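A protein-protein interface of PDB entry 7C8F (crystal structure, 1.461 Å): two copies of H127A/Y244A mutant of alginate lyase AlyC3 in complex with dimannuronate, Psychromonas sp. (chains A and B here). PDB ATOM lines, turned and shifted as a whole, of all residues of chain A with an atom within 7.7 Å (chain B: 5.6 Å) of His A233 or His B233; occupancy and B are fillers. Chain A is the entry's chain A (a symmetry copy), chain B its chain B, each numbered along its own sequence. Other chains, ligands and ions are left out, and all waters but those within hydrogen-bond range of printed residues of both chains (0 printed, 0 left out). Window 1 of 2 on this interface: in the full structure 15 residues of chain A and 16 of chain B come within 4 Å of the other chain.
The side-chain carboxylate of Asp B89 lies within salt-bridge range of the guanidinium group of Arg A232 (3.0 Å). OD2 of Asp B229 is in salt-bridge range of NH1 of Arg A87 (2.8 Å). The guanidinium group (NE) of Arg B232 is in salt-bridge range of the side-chain carboxylate (OD2) of Asp A89, 2.9 Å away. O of Arg B232 is in hydrogen-bond range of NH2 of Arg A232, at 2.9 Å. NH2 of Arg A87 sits close to NE of Arg B232, at 3.2 Å.
OD1 of Asp B229 is in salt-bridge range of NH1 of Arg B232 (3.5 Å). OD2 of Asp A89 is in salt-bridge range of NH2 of Arg A87. The backbone NH (N) of Leu A130 sits at hydrogen-bond distance from the backbone carbonyl oxygen (O) of Thr A135 (2.8 Å). The side-chain carboxylate (OD2) of Asp A229 is in salt-bridge range of the guanidinium group (NH1) of Arg A232, at 3.4 Å.
O of Ala B166 touches CD1 of Leu A130, 3.8 Å away. O of Ala A166 touches CD1 of Leu B130 (3.8 Å). His B233 touches Arg A232. His A233 touches Arg B232. CG of His B233 touches CG of His A233, at 3.4 Å.
Gly A129 touches none of the printed residues of chain B. Printed residues of chain B within 4 Å of Ala A166: Leu B130. His A233 touches just these residues of chain B: Arg B232 (3.6 Å) and His B233 (3.4 Å). Of the printed residues of chain A, Asp B89 touches Arg A232 (3.0 Å). Printed residues of chain A within 4 Å of Leu B130: Ala A166 (3.8 Å). Printed residues of chain A within 4 Å of His B233: Arg A232 (3.6 Å) and His A233 (3.4 Å).
Of the 23 printed residues of chain A, 6 touch a printed residue of chain B. Hydrophobic or aromatic side chains of chain A within 4 Å of the printed part of chain B: Leu A130 and His A233. Hydrophobic or aromatic side chains of chain B that line the printed part of chain A: Leu B130 and His B233. Among the printed residues, 10 pairs touch across the chains. Among the printed residues, Asp or Glu carboxylates within 4 Å of a Lys or Arg side-chain nitrogen of the other chain: Arg A87 with Asp B229, Asp A89 with Arg B232 and Arg A232 with Asp B89.
Asp A89 touches Arg B232, and with the chains exchanged Arg A232 touches Asp B89. Leu A130 touches Ala B166, and with the chains exchanged Ala A166 touches Leu B130. Arg A232 touches His B233, and with the chains exchanged His A233 touches Arg B232. His A233 touches its own counterpart, His B233. 12 positions are printed for both chains.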
ATOM      1  N   PHE A  86      23.475   6.443  10.819  1.00  0.00           N
ATOM      2  CA  PHE A  86      22.074   6.152  10.989  1.00  0.00           C
ATOM      3  C   PHE A  86      21.186   6.401   9.802  1.00  0.00           C
ATOM      4  O   PHE A  86      21.461   7.177   8.985  1.00  0.00           O
ATOM      5  CB  PHE A  86      21.501   6.919  12.216  1.00  0.00           C
ATOM      6  CG  PHE A  86      21.848   8.400  12.276  1.00  0.00           C
ATOM      7  CD1 PHE A  86      21.183   9.309  11.511  1.00  0.00           C
ATOM      8  CD2 PHE A  86      22.840   8.857  13.091  1.00  0.00           C
ATOM      9  CE1 PHE A  86      21.494  10.640  11.544  1.00  0.00           C
ATOM     10  CE2 PHE A  86      23.160  10.211  13.136  1.00  0.00           C
ATOM     11  CZ  PHE A  86      22.481  11.097  12.362  1.00  0.00           C
ATOM     12  N   ARG A  87      20.083   5.684   9.792  1.00  0.00           N
ATOM     13  CA  ARG A  87      19.041   5.881   8.810  1.00  0.00           C
ATOM     14  C   ARG A  87      18.250   7.101   9.250  1.00  0.00           C
ATOM     15  O   ARG A  87      18.070   7.304  10.387  1.00  0.00           O
ATOM     16  CB  ARG A  87      18.131   4.660   8.720  1.00  0.00           C
ATOM     17  CG  ARG A  87      18.774   3.612   7.854  1.00  0.00           C
ATOM     18  CD  ARG A  87      17.874   2.503   7.486  1.00  0.00           C
ATOM     19  NE  ARG A  87      16.764   2.861   6.630  1.00  0.00           N
ATOM     20  CZ  ARG A  87      16.108   1.957   5.951  1.00  0.00           C
ATOM     21  NH1 ARG A  87      16.484   0.693   6.014  1.00  0.00           N
ATOM     22  NH2 ARG A  87      15.127   2.305   5.207  1.00  0.00           N
ATOM     23  N   THR A  88      17.813   7.894   8.301  1.00  0.00           N
ATOM     24  CA  THR A  88      17.088   9.129   8.573  1.00  0.00           C
ATOM     25  C   THR A  88      15.605   9.009   8.265  1.00  0.00           C
ATOM     26  O   THR A  88      14.860   9.979   8.485  1.00  0.00           O
ATOM     27  CB  THR A  88      17.680  10.299   7.760  1.00  0.00           C
ATOM     28  OG1 THR A  88      17.378  10.123   6.362  1.00  0.00           O
ATOM     29  CG2 THR A  88      19.191  10.405   7.956  1.00  0.00           C
ATOM     30  N   ASP A  89      15.160   7.858   7.755  1.00  0.00           N
ATOM     31  CA  ASP A  89      13.842   7.711   7.149  1.00  0.00           C
ATOM     32  C   ASP A  89      12.876   6.836   7.942  1.00  0.00           C
ATOM     33  O   ASP A  89      11.746   6.617   7.479  1.00  0.00           O
ATOM     34  CB  ASP A  89      13.984   7.157   5.721  1.00  0.00           C
ATOM     35  CG  ASP A  89      14.735   5.816   5.657  1.00  0.00           C
ATOM     36  OD1 ASP A  89      15.594   5.509   6.523  1.00  0.00           O
ATOM     37  OD2 ASP A  89      14.446   5.051   4.705  1.00  0.00           O
ATOM     38  N   ASN A 127      26.525  12.704   5.266  1.00  0.00           N
ATOM     39  CA  ASN A 127      26.201  11.337   4.873  1.00  0.00           C
ATOM     40  C   ASN A 127      27.481  10.543   4.711  1.00  0.00           C
ATOM     41  O   ASN A 127      28.502  11.067   4.246  1.00  0.00           O
ATOM     42  CB  ASN A 127      25.346  11.218   3.592  1.00  0.00           C
ATOM     43  CG  ASN A 127      26.122  11.555   2.323  1.00  0.00           C
ATOM     44  OD1 ASN A 127      26.607  10.670   1.611  1.00  0.00           O
ATOM     45  ND2 ASN A 127      26.236  12.850   2.036  1.00  0.00           N
ATOM     46  N   GLY A 129      27.072   7.408   3.021  1.00  0.00           N
ATOM     47  CA  GLY A 129      26.742   6.900   1.705  1.00  0.00           C
ATOM     48  C   GLY A 129      25.623   5.882   1.835  1.00  0.00           C
ATOM     49  O   GLY A 129      24.825   5.947   2.766  1.00  0.00           O
ATOM     50  N   LEU A 130      25.593   4.930   0.897  1.00  0.00           N
ATOM     51  CA  LEU A 130      24.545   3.914   0.940  1.00  0.00           C
ATOM     52  C   LEU A 130      24.780   2.888   2.042  1.00  0.00           C
ATOM     53  O   LEU A 130      23.832   2.200   2.438  1.00  0.00           O
ATOM     54  CB  LEU A 130      24.477   3.145  -0.383  1.00  0.00           C
ATOM     55  CG  LEU A 130      23.978   3.915  -1.594  1.00  0.00           C
ATOM     56  CD1 LEU A 130      24.173   3.039  -2.830  1.00  0.00           C
ATOM     57  CD2 LEU A 130      22.520   4.349  -1.423  1.00  0.00           C
ATOM     58  N   ASP A 131      26.014   2.769   2.538  1.00  0.00           N
ATOM     59  CA  ASP A 131      26.399   1.736   3.490  1.00  0.00           C
ATOM     60  C   ASP A 131      27.479   2.309   4.397  1.00  0.00           C
ATOM     61  O   ASP A 131      27.915   3.451   4.220  1.00  0.00           O
ATOM     62  CB  ASP A 131      26.858   0.465   2.760  1.00  0.00           C
ATOM     63  CG  ASP A 131      27.974   0.730   1.759  1.00  0.00           C
ATOM     64  OD1 ASP A 131      28.761   1.673   1.959  1.00  0.00           O
ATOM     65  OD2 ASP A 131      28.065  -0.014   0.757  1.00  0.00           O
ATOM     66  N   THR A 135      29.819   3.728   0.171  1.00  0.00           N
ATOM     67  CA  THR A 135      29.524   3.559  -1.243  1.00  0.00           C
ATOM     68  C   THR A 135      28.579   4.655  -1.722  1.00  0.00           C
ATOM     69  O   THR A 135      27.576   4.963  -1.070  1.00  0.00           O
ATOM     70  CB  THR A 135      28.886   2.189  -1.456  1.00  0.00           C
ATOM     71  OG1 THR A 135      29.732   1.187  -0.869  1.00  0.00           O
ATOM     72  CG2 THR A 135      28.709   1.895  -2.937  1.00  0.00           C
ATOM     73  N   HIS A 136      28.907   5.252  -2.864  1.00  0.00           N
ATOM     74  CA  HIS A 136      28.091   6.313  -3.458  1.00  0.00           C
ATOM     75  C   HIS A 136      27.868   7.482  -2.493  1.00  0.00           C
ATOM     76  O   HIS A 136      26.781   8.062  -2.418  1.00  0.00           O
ATOM     77  CB  HIS A 136      26.785   5.768  -4.041  1.00  0.00           C
ATOM     78  CG  HIS A 136      26.990   4.927  -5.264  1.00  0.00           C
ATOM     79  ND1 HIS A 136      27.667   5.390  -6.370  1.00  0.00           N
ATOM     80  CD2 HIS A 136      26.637   3.650  -5.545  1.00  0.00           C
ATOM     81  CE1 HIS A 136      27.707   4.440  -7.289  1.00  0.00           C
ATOM     82  NE2 HIS A 136      27.086   3.374  -6.816  1.00  0.00           N
ATOM     83  N   VAL A 138      27.691  11.111  -1.172  1.00  0.00           N
ATOM     84  CA  VAL A 138      27.340  12.395  -1.769  1.00  0.00           C
ATOM     85  C   VAL A 138      28.199  13.455  -1.083  1.00  0.00           C
ATOM     86  O   VAL A 138      28.134  13.576   0.145  1.00  0.00           O
ATOM     87  CB  VAL A 138      25.847  12.693  -1.586  1.00  0.00           C
ATOM     88  CG1 VAL A 138      25.501  14.107  -2.037  1.00  0.00           C
ATOM     89  CG2 VAL A 138      25.018  11.659  -2.372  1.00  0.00           C
ATOM     90  N   ASN A 165      18.377  18.221  -1.881  1.00  0.00           N
ATOM     91  CA  ASN A 165      18.207  17.062  -2.749  1.00  0.00           C
ATOM     92  C   ASN A 165      19.371  16.127  -2.454  1.00  0.00           C
ATOM     93  O   ASN A 165      20.216  16.420  -1.599  1.00  0.00           O
ATOM     94  CB  ASN A 165      18.043  17.477  -4.225  1.00  0.00           C
ATOM     95  CG  ASN A 165      19.248  18.234  -4.783  1.00  0.00           C
ATOM     96  OD1 ASN A 165      20.388  17.949  -4.447  1.00  0.00           O
ATOM     97  ND2 ASN A 165      18.974  19.206  -5.667  1.00  0.00           N
ATOM     98  N   ALA A 166      19.410  14.985  -3.152  1.00  0.00           N
ATOM     99  CA  ALA A 166      20.489  14.021  -2.956  1.00  0.00           C
ATOM    100  C   ALA A 166      21.435  13.960  -4.157  1.00  0.00           C
ATOM    101  O   ALA A 166      22.039  12.919  -4.437  1.00  0.00           O
ATOM    102  CB  ALA A 166      19.927  12.640  -2.608  1.00  0.00           C
ATOM    103  N   VAL A 167      21.574  15.072  -4.869  1.00  0.00           N
ATOM    104  CA  VAL A 167      22.311  15.109  -6.130  1.00  0.00           C
ATOM    105  C   VAL A 167      23.765  15.494  -5.894  1.00  0.00           C
ATOM    106  O   VAL A 167      24.070  16.402  -5.109  1.00  0.00           O
ATOM    107  CB  VAL A 167      21.634  16.091  -7.098  1.00  0.00           C
ATOM    108  CG1 VAL A 167      22.423  16.175  -8.401  1.00  0.00           C
ATOM    109  CG2 VAL A 167      20.190  15.672  -7.361  1.00  0.00           C
ATOM    110  N   ILE A 228      12.911  15.398   4.718  1.00  0.00           N
ATOM    111  CA  ILE A 228      14.108  14.862   4.098  1.00  0.00           C
ATOM    112  C   ILE A 228      13.904  13.490   3.471  1.00  0.00           C
ATOM    113  O   ILE A 228      14.796  12.746   3.326  1.00  0.00           O
ATOM    114  CB  ILE A 228      15.317  14.822   5.033  1.00  0.00           C
ATOM    115  CG1 ILE A 228      15.009  14.034   6.305  1.00  0.00           C
ATOM    116  CG2 ILE A 228      15.749  16.235   5.375  1.00  0.00           C
ATOM    117  CD1 ILE A 228      16.221  13.704   7.146  1.00  0.00           C
ATOM    118  N   ASP A 229      12.724  13.270   2.924  1.00  0.00           N
ATOM    119  CA  ASP A 229      12.394  12.033   2.190  1.00  0.00           C
ATOM    120  C   ASP A 229      13.425  11.772   1.062  1.00  0.00           C
ATOM    121  O   ASP A 229      13.806  10.692   0.834  1.00  0.00           O
ATOM    122  CB  ASP A 229      10.981  12.194   1.611  1.00  0.00           C
ATOM    123  CG  ASP A 229      10.350  10.917   1.081  1.00  0.00           C
ATOM    124  OD1 ASP A 229       9.362  11.113   0.441  1.00  0.00           O
ATOM    125  OD2 ASP A 229      10.783   9.853   1.315  1.00  0.00           O
ATOM    126  N   TYR A 230      13.850  12.817   0.386  1.00  0.00           N
ATOM    127  CA  TYR A 230      14.863  12.732  -0.651  1.00  0.00           C
ATOM    128  C   TYR A 230      16.218  12.142  -0.239  1.00  0.00           C
ATOM    129  O   TYR A 230      16.899  11.711  -1.067  1.00  0.00           O
ATOM    130  CB  TYR A 230      15.087  14.119  -1.307  1.00  0.00           C
ATOM    131  CG  TYR A 230      15.583  15.186  -0.350  1.00  0.00           C
ATOM    132  CD1 TYR A 230      16.911  15.328  -0.063  1.00  0.00           C
ATOM    133  CD2 TYR A 230      14.714  16.026   0.250  1.00  0.00           C
ATOM    134  CE1 TYR A 230      17.350  16.284   0.819  1.00  0.00           C
ATOM    135  CE2 TYR A 230      15.143  16.993   1.131  1.00  0.00           C
ATOM    136  CZ  TYR A 230      16.455  17.105   1.416  1.00  0.00           C
ATOM    137  OH  TYR A 230      16.873  18.059   2.277  1.00  0.00           O
ATOM    138  N   TRP A 231      16.544  12.175   1.046  1.00  0.00           N
ATOM    139  CA  TRP A 231      17.777  11.690   1.611  1.00  0.00           C
ATOM    140  C   TRP A 231      17.682  10.279   2.194  1.00  0.00           C
ATOM    141  O   TRP A 231      18.614   9.798   2.694  1.00  0.00           O
ATOM    142  CB  TRP A 231      18.141  12.646   2.751  1.00  0.00           C
ATOM    143  CG  TRP A 231      19.578  12.735   3.174  1.00  0.00           C
ATOM    144  CD1 TRP A 231      20.124  12.199   4.268  1.00  0.00           C
ATOM    145  CD2 TRP A 231      20.614  13.472   2.532  1.00  0.00           C
ATOM    146  NE1 TRP A 231      21.425  12.521   4.358  1.00  0.00           N
ATOM    147  CE2 TRP A 231      21.755  13.319   3.302  1.00  0.00           C
ATOM    148  CE3 TRP A 231      20.677  14.263   1.391  1.00  0.00           C
ATOM    149  CZ2 TRP A 231      22.966  13.925   2.960  1.00  0.00           C
ATOM    150  CZ3 TRP A 231      21.878  14.834   1.054  1.00  0.00           C
ATOM    151  CH2 TRP A 231      22.994  14.671   1.839  1.00  0.00           C
ATOM    152  N   ARG A 232      16.551   9.638   1.987  1.00  0.00           N
ATOM    153  CA  ARG A 232      16.267   8.399   2.665  1.00  0.00           C
ATOM    154  C   ARG A 232      17.240   7.268   2.537  1.00  0.00           C
ATOM    155  O   ARG A 232      17.388   6.518   3.444  1.00  0.00           O
ATOM    156  CB  ARG A 232      14.843   7.927   2.333  1.00  0.00           C
ATOM    157  CG  ARG A 232      14.617   7.565   0.881  1.00  0.00           C
ATOM    158  CD  ARG A 232      13.141   7.392   0.591  1.00  0.00           C
ATOM    159  NE  ARG A 232      12.808   7.099  -0.799  1.00  0.00           N
ATOM    160  CZ  ARG A 232      12.579   8.006  -1.721  1.00  0.00           C
ATOM    161  NH1 ARG A 232      12.722   9.282  -1.466  1.00  0.00           N
ATOM    162  NH2 ARG A 232      12.226   7.641  -2.919  1.00  0.00           N
ATOM    163  N   HIS A 233      17.908   7.201   1.402  1.00  0.00           N
ATOM    164  CA  HIS A 233      18.855   6.121   1.134  1.00  0.00           C
ATOM    165  C   HIS A 233      20.218   6.353   1.761  1.00  0.00           C
ATOM    166  O   HIS A 233      21.050   5.439   1.756  1.00  0.00           O
ATOM    167  CB  HIS A 233      19.040   5.957  -0.376  1.00  0.00           C
ATOM    168  CG  HIS A 233      19.386   7.235  -1.072  1.00  0.00           C
ATOM    169  ND1 HIS A 233      18.613   8.373  -0.970  1.00  0.00           N
ATOM    170  CD2 HIS A 233      20.438   7.559  -1.866  1.00  0.00           C
ATOM    171  CE1 HIS A 233      19.152   9.333  -1.698  1.00  0.00           C
ATOM    172  NE2 HIS A 233      20.265   8.867  -2.249  1.00  0.00           N
ATOM    173  N   LEU A 234      20.484   7.542   2.292  1.00  0.00           N
ATOM    174  CA  LEU A 234      21.824   7.910   2.735  1.00  0.00           C
ATOM    175  C   LEU A 234      21.962   7.759   4.244  1.00  0.00           C
ATOM    176  O   LEU A 234      21.298   8.464   5.012  1.00  0.00           O
ATOM    177  CB  LEU A 234      22.138   9.344   2.304  1.00  0.00           C
ATOM    178  CG  LEU A 234      22.175   9.522   0.777  1.00  0.00           C
ATOM    179  CD1 LEU A 234      22.270  11.006   0.412  1.00  0.00           C
ATOM    180  CD2 LEU A 234      23.345   8.740   0.173  1.00  0.00           C
ATOM    181  N   LEU A 235      22.836   6.849   4.659  1.00  0.00           N
ATOM    182  CA  LEU A 235      23.197   6.751   6.066  1.00  0.00           C
ATOM    183  C   LEU A 235      23.984   7.993   6.462  1.00  0.00           C
ATOM    184  O   LEU A 235      24.867   8.449   5.724  1.00  0.00           O
ATOM    185  CB  LEU A 235      24.065   5.523   6.315  1.00  0.00           C
ATOM    186  CG  LEU A 235      23.459   4.171   5.939  1.00  0.00           C
ATOM    187  CD1 LEU A 235      24.470   3.076   6.291  1.00  0.00           C
ATOM    188  CD2 LEU A 235      22.141   3.946   6.662  1.00  0.00           C
ATOM    189  N   SER A 236      23.647   8.557   7.614  1.00  0.00           N
ATOM    190  CA  SER A 236      24.080   9.900   7.969  1.00  0.00           C
ATOM    191  C   SER A 236      24.695   9.894   9.363  1.00  0.00           C
ATOM    192  O   SER A 236      24.562   8.924  10.117  1.00  0.00           O
ATOM    193  CB  SER A 236      22.888  10.859   7.896  1.00  0.00           C
ATOM    194  OG  SER A 236      22.383  10.875   6.558  1.00  0.00           O
ATOM    195  N   ASP B  89       8.721   2.011  -2.494  1.00  0.00           N
ATOM    196  CA  ASP B  89       8.943   1.907  -1.060  1.00  0.00           C
ATOM    197  C   ASP B  89       7.736   2.286  -0.217  1.00  0.00           C
ATOM    198  O   ASP B  89       7.846   2.290   1.012  1.00  0.00           O
ATOM    199  CB  ASP B  89      10.161   2.753  -0.648  1.00  0.00           C
ATOM    200  CG  ASP B  89      10.048   4.230  -1.054  1.00  0.00           C
ATOM    201  OD1 ASP B  89       9.403   4.573  -2.072  1.00  0.00           O
ATOM    202  OD2 ASP B  89      10.635   5.072  -0.328  1.00  0.00           O
ATOM    203  N   GLY B 129      15.944   6.594 -12.018  1.00  0.00           N
ATOM    204  CA  GLY B 129      16.951   7.263 -11.205  1.00  0.00           C
ATOM    205  C   GLY B 129      16.280   7.903 -10.002  1.00  0.00           C
ATOM    206  O   GLY B 129      15.229   7.449  -9.557  1.00  0.00           O
ATOM    207  N   LEU B 130      16.893   8.974  -9.490  1.00  0.00           N
ATOM    208  CA  LEU B 130      16.311   9.644  -8.331  1.00  0.00           C
ATOM    209  C   LEU B 130      15.071  10.449  -8.685  1.00  0.00           C
ATOM    210  O   LEU B 130      14.284  10.767  -7.785  1.00  0.00           O
ATOM    211  CB  LEU B 130      17.316  10.620  -7.733  1.00  0.00           C
ATOM    212  CG  LEU B 130      18.552  10.015  -7.082  1.00  0.00           C
ATOM    213  CD1 LEU B 130      19.488  11.145  -6.706  1.00  0.00           C
ATOM    214  CD2 LEU B 130      18.203   9.187  -5.839  1.00  0.00           C
ATOM    215  N   VAL B 138      20.968   4.143 -12.078  1.00  0.00           N
ATOM    216  CA  VAL B 138      21.781   2.955 -11.833  1.00  0.00           C
ATOM    217  C   VAL B 138      21.639   2.051 -13.056  1.00  0.00           C
ATOM    218  O   VAL B 138      20.509   1.699 -13.417  1.00  0.00           O
ATOM    219  CB  VAL B 138      21.339   2.243 -10.545  1.00  0.00           C
ATOM    220  CG1 VAL B 138      22.064   0.910 -10.364  1.00  0.00           C
ATOM    221  CG2 VAL B 138      21.602   3.164  -9.352  1.00  0.00           C
ATOM    222  N   ALA B 166      21.833  -1.301  -4.524  1.00  0.00           N
ATOM    223  CA  ALA B 166      21.650  -0.146  -5.399  1.00  0.00           C
ATOM    224  C   ALA B 166      22.982   0.398  -5.912  1.00  0.00           C
ATOM    225  O   ALA B 166      23.106   1.592  -6.209  1.00  0.00           O
ATOM    226  CB  ALA B 166      20.820   0.936  -4.713  1.00  0.00           C
ATOM    227  N   ASP B 229      14.096  -2.787   0.192  1.00  0.00           N
ATOM    228  CA  ASP B 229      14.342  -1.552   0.953  1.00  0.00           C
ATOM    229  C   ASP B 229      15.556  -0.795   0.363  1.00  0.00           C
ATOM    230  O   ASP B 229      15.563   0.383   0.297  1.00  0.00           O
ATOM    231  CB  ASP B 229      14.603  -1.945   2.419  1.00  0.00           C
ATOM    232  CG  ASP B 229      14.570  -0.802   3.425  1.00  0.00           C
ATOM    233  OD1 ASP B 229      14.146   0.252   3.154  1.00  0.00           O
ATOM    234  OD2 ASP B 229      14.940  -1.103   4.523  1.00  0.00           O
ATOM    235  N   TYR B 230      16.553  -1.538  -0.045  1.00  0.00           N
ATOM    236  CA  TYR B 230      17.766  -0.966  -0.612  1.00  0.00           C
ATOM    237  C   TYR B 230      17.591  -0.112  -1.869  1.00  0.00           C
ATOM    238  O   TYR B 230      18.431   0.654  -2.182  1.00  0.00           O
ATOM    239  CB  TYR B 230      18.803  -2.071  -0.911  1.00  0.00           C
ATOM    240  CG  TYR B 230      18.321  -3.149  -1.867  1.00  0.00           C
ATOM    241  CD1 TYR B 230      18.410  -2.973  -3.220  1.00  0.00           C
ATOM    242  CD2 TYR B 230      17.779  -4.315  -1.394  1.00  0.00           C
ATOM    243  CE1 TYR B 230      17.944  -3.915  -4.077  1.00  0.00           C
ATOM    244  CE2 TYR B 230      17.323  -5.272  -2.239  1.00  0.00           C
ATOM    245  CZ  TYR B 230      17.398  -5.060  -3.567  1.00  0.00           C
ATOM    246  OH  TYR B 230      16.953  -6.035  -4.392  1.00  0.00           O
ATOM    247  N   TRP B 231      16.474  -0.302  -2.548  1.00  0.00           N
ATOM    248  CA  TRP B 231      16.143   0.375  -3.783  1.00  0.00           C
ATOM    249  C   TRP B 231      15.201   1.560  -3.614  1.00  0.00           C
ATOM    250  O   TRP B 231      14.791   2.138  -4.544  1.00  0.00           O
ATOM    251  CB  TRP B 231      15.431  -0.644  -4.661  1.00  0.00           C
ATOM    252  CG  TRP B 231      15.404  -0.455  -6.150  1.00  0.00           C
ATOM    253  CD1 TRP B 231      14.371  -0.051  -6.891  1.00  0.00           C
ATOM    254  CD2 TRP B 231      16.451  -0.751  -7.054  1.00  0.00           C
ATOM    255  NE1 TRP B 231      14.689  -0.045  -8.206  1.00  0.00           N
ATOM    256  CE2 TRP B 231      15.976  -0.481  -8.338  1.00  0.00           C
ATOM    257  CE3 TRP B 231      17.754  -1.219  -6.903  1.00  0.00           C
ATOM    258  CZ2 TRP B 231      16.760  -0.672  -9.457  1.00  0.00           C
ATOM    259  CZ3 TRP B 231      18.510  -1.393  -8.007  1.00  0.00           C
ATOM    260  CH2 TRP B 231      18.009  -1.130  -9.262  1.00  0.00           C
ATOM    261  N   ARG B 232      14.884   1.862  -2.384  1.00  0.00           N
ATOM    262  CA  ARG B 232      13.869   2.861  -2.057  1.00  0.00           C
ATOM    263  C   ARG B 232      13.930   4.220  -2.706  1.00  0.00           C
ATOM    264  O   ARG B 232      12.897   4.790  -2.985  1.00  0.00           O
ATOM    265  CB  ARG B 232      13.716   2.998  -0.538  1.00  0.00           C
ATOM    266  CG  ARG B 232      14.909   3.552   0.203  1.00  0.00           C
ATOM    267  CD  ARG B 232      14.787   3.359   1.704  1.00  0.00           C
ATOM    268  NE  ARG B 232      15.911   3.850   2.488  1.00  0.00           N
ATOM    269  CZ  ARG B 232      16.982   3.140   2.766  1.00  0.00           C
ATOM    270  NH1 ARG B 232      17.132   1.943   2.296  1.00  0.00           N
ATOM    271  NH2 ARG B 232      17.920   3.624   3.513  1.00  0.00           N
ATOM    272  N   HIS B 233      15.146   4.683  -2.932  1.00  0.00           N
ATOM    273  CA  HIS B 233      15.332   6.004  -3.535  1.00  0.00           C
ATOM    274  C   HIS B 233      15.156   6.022  -5.050  1.00  0.00           C
ATOM    275  O   HIS B 233      15.138   7.114  -5.637  1.00  0.00           O
ATOM    276  CB  HIS B 233      16.739   6.526  -3.221  1.00  0.00           C
ATOM    277  CG  HIS B 233      17.828   5.569  -3.610  1.00  0.00           C
ATOM    278  ND1 HIS B 233      17.866   4.271  -3.153  1.00  0.00           N
ATOM    279  CD2 HIS B 233      18.914   5.722  -4.409  1.00  0.00           C
ATOM    280  CE1 HIS B 233      18.936   3.665  -3.639  1.00  0.00           C
ATOM    281  NE2 HIS B 233      19.598   4.526  -4.393  1.00  0.00           N
ATOM    282  N   LEU B 234      15.033   4.867  -5.703  1.00  0.00           N
ATOM    283  CA  LEU B 234      15.059   4.804  -7.162  1.00  0.00           C
ATOM    284  C   LEU B 234      13.643   4.689  -7.723  1.00  0.00           C
ATOM    285  O   LEU B 234      12.954   3.691  -7.493  1.00  0.00           O
ATOM    286  CB  LEU B 234      15.932   3.631  -7.613  1.00  0.00           C
ATOM    287  CG  LEU B 234      17.405   3.795  -7.223  1.00  0.00           C
ATOM    288  CD1 LEU B 234      18.156   2.488  -7.467  1.00  0.00           C
ATOM    289  CD2 LEU B 234      18.027   4.942  -8.022  1.00  0.00           C
ATOM    290  N   LEU B 235      13.214   5.707  -8.466  1.00  0.00           N
ATOM    291  CA  LEU B 235      11.970   5.594  -9.218  1.00  0.00           C
ATOM    292  C   LEU B 235      12.132   4.534 -10.296  1.00  0.00           C
ATOM    293  O   LEU B 235      13.164   4.472 -10.973  1.00  0.00           O
ATOM    294  CB  LEU B 235      11.631   6.936  -9.869  1.00  0.00           C
ATOM    295  CG  LEU B 235      11.437   8.116  -8.913  1.00  0.00           C
ATOM    296  CD1 LEU B 235      11.022   9.365  -9.689  1.00  0.00           C
ATOM    297  CD2 LEU B 235      10.398   7.790  -7.840  1.00  0.00           C
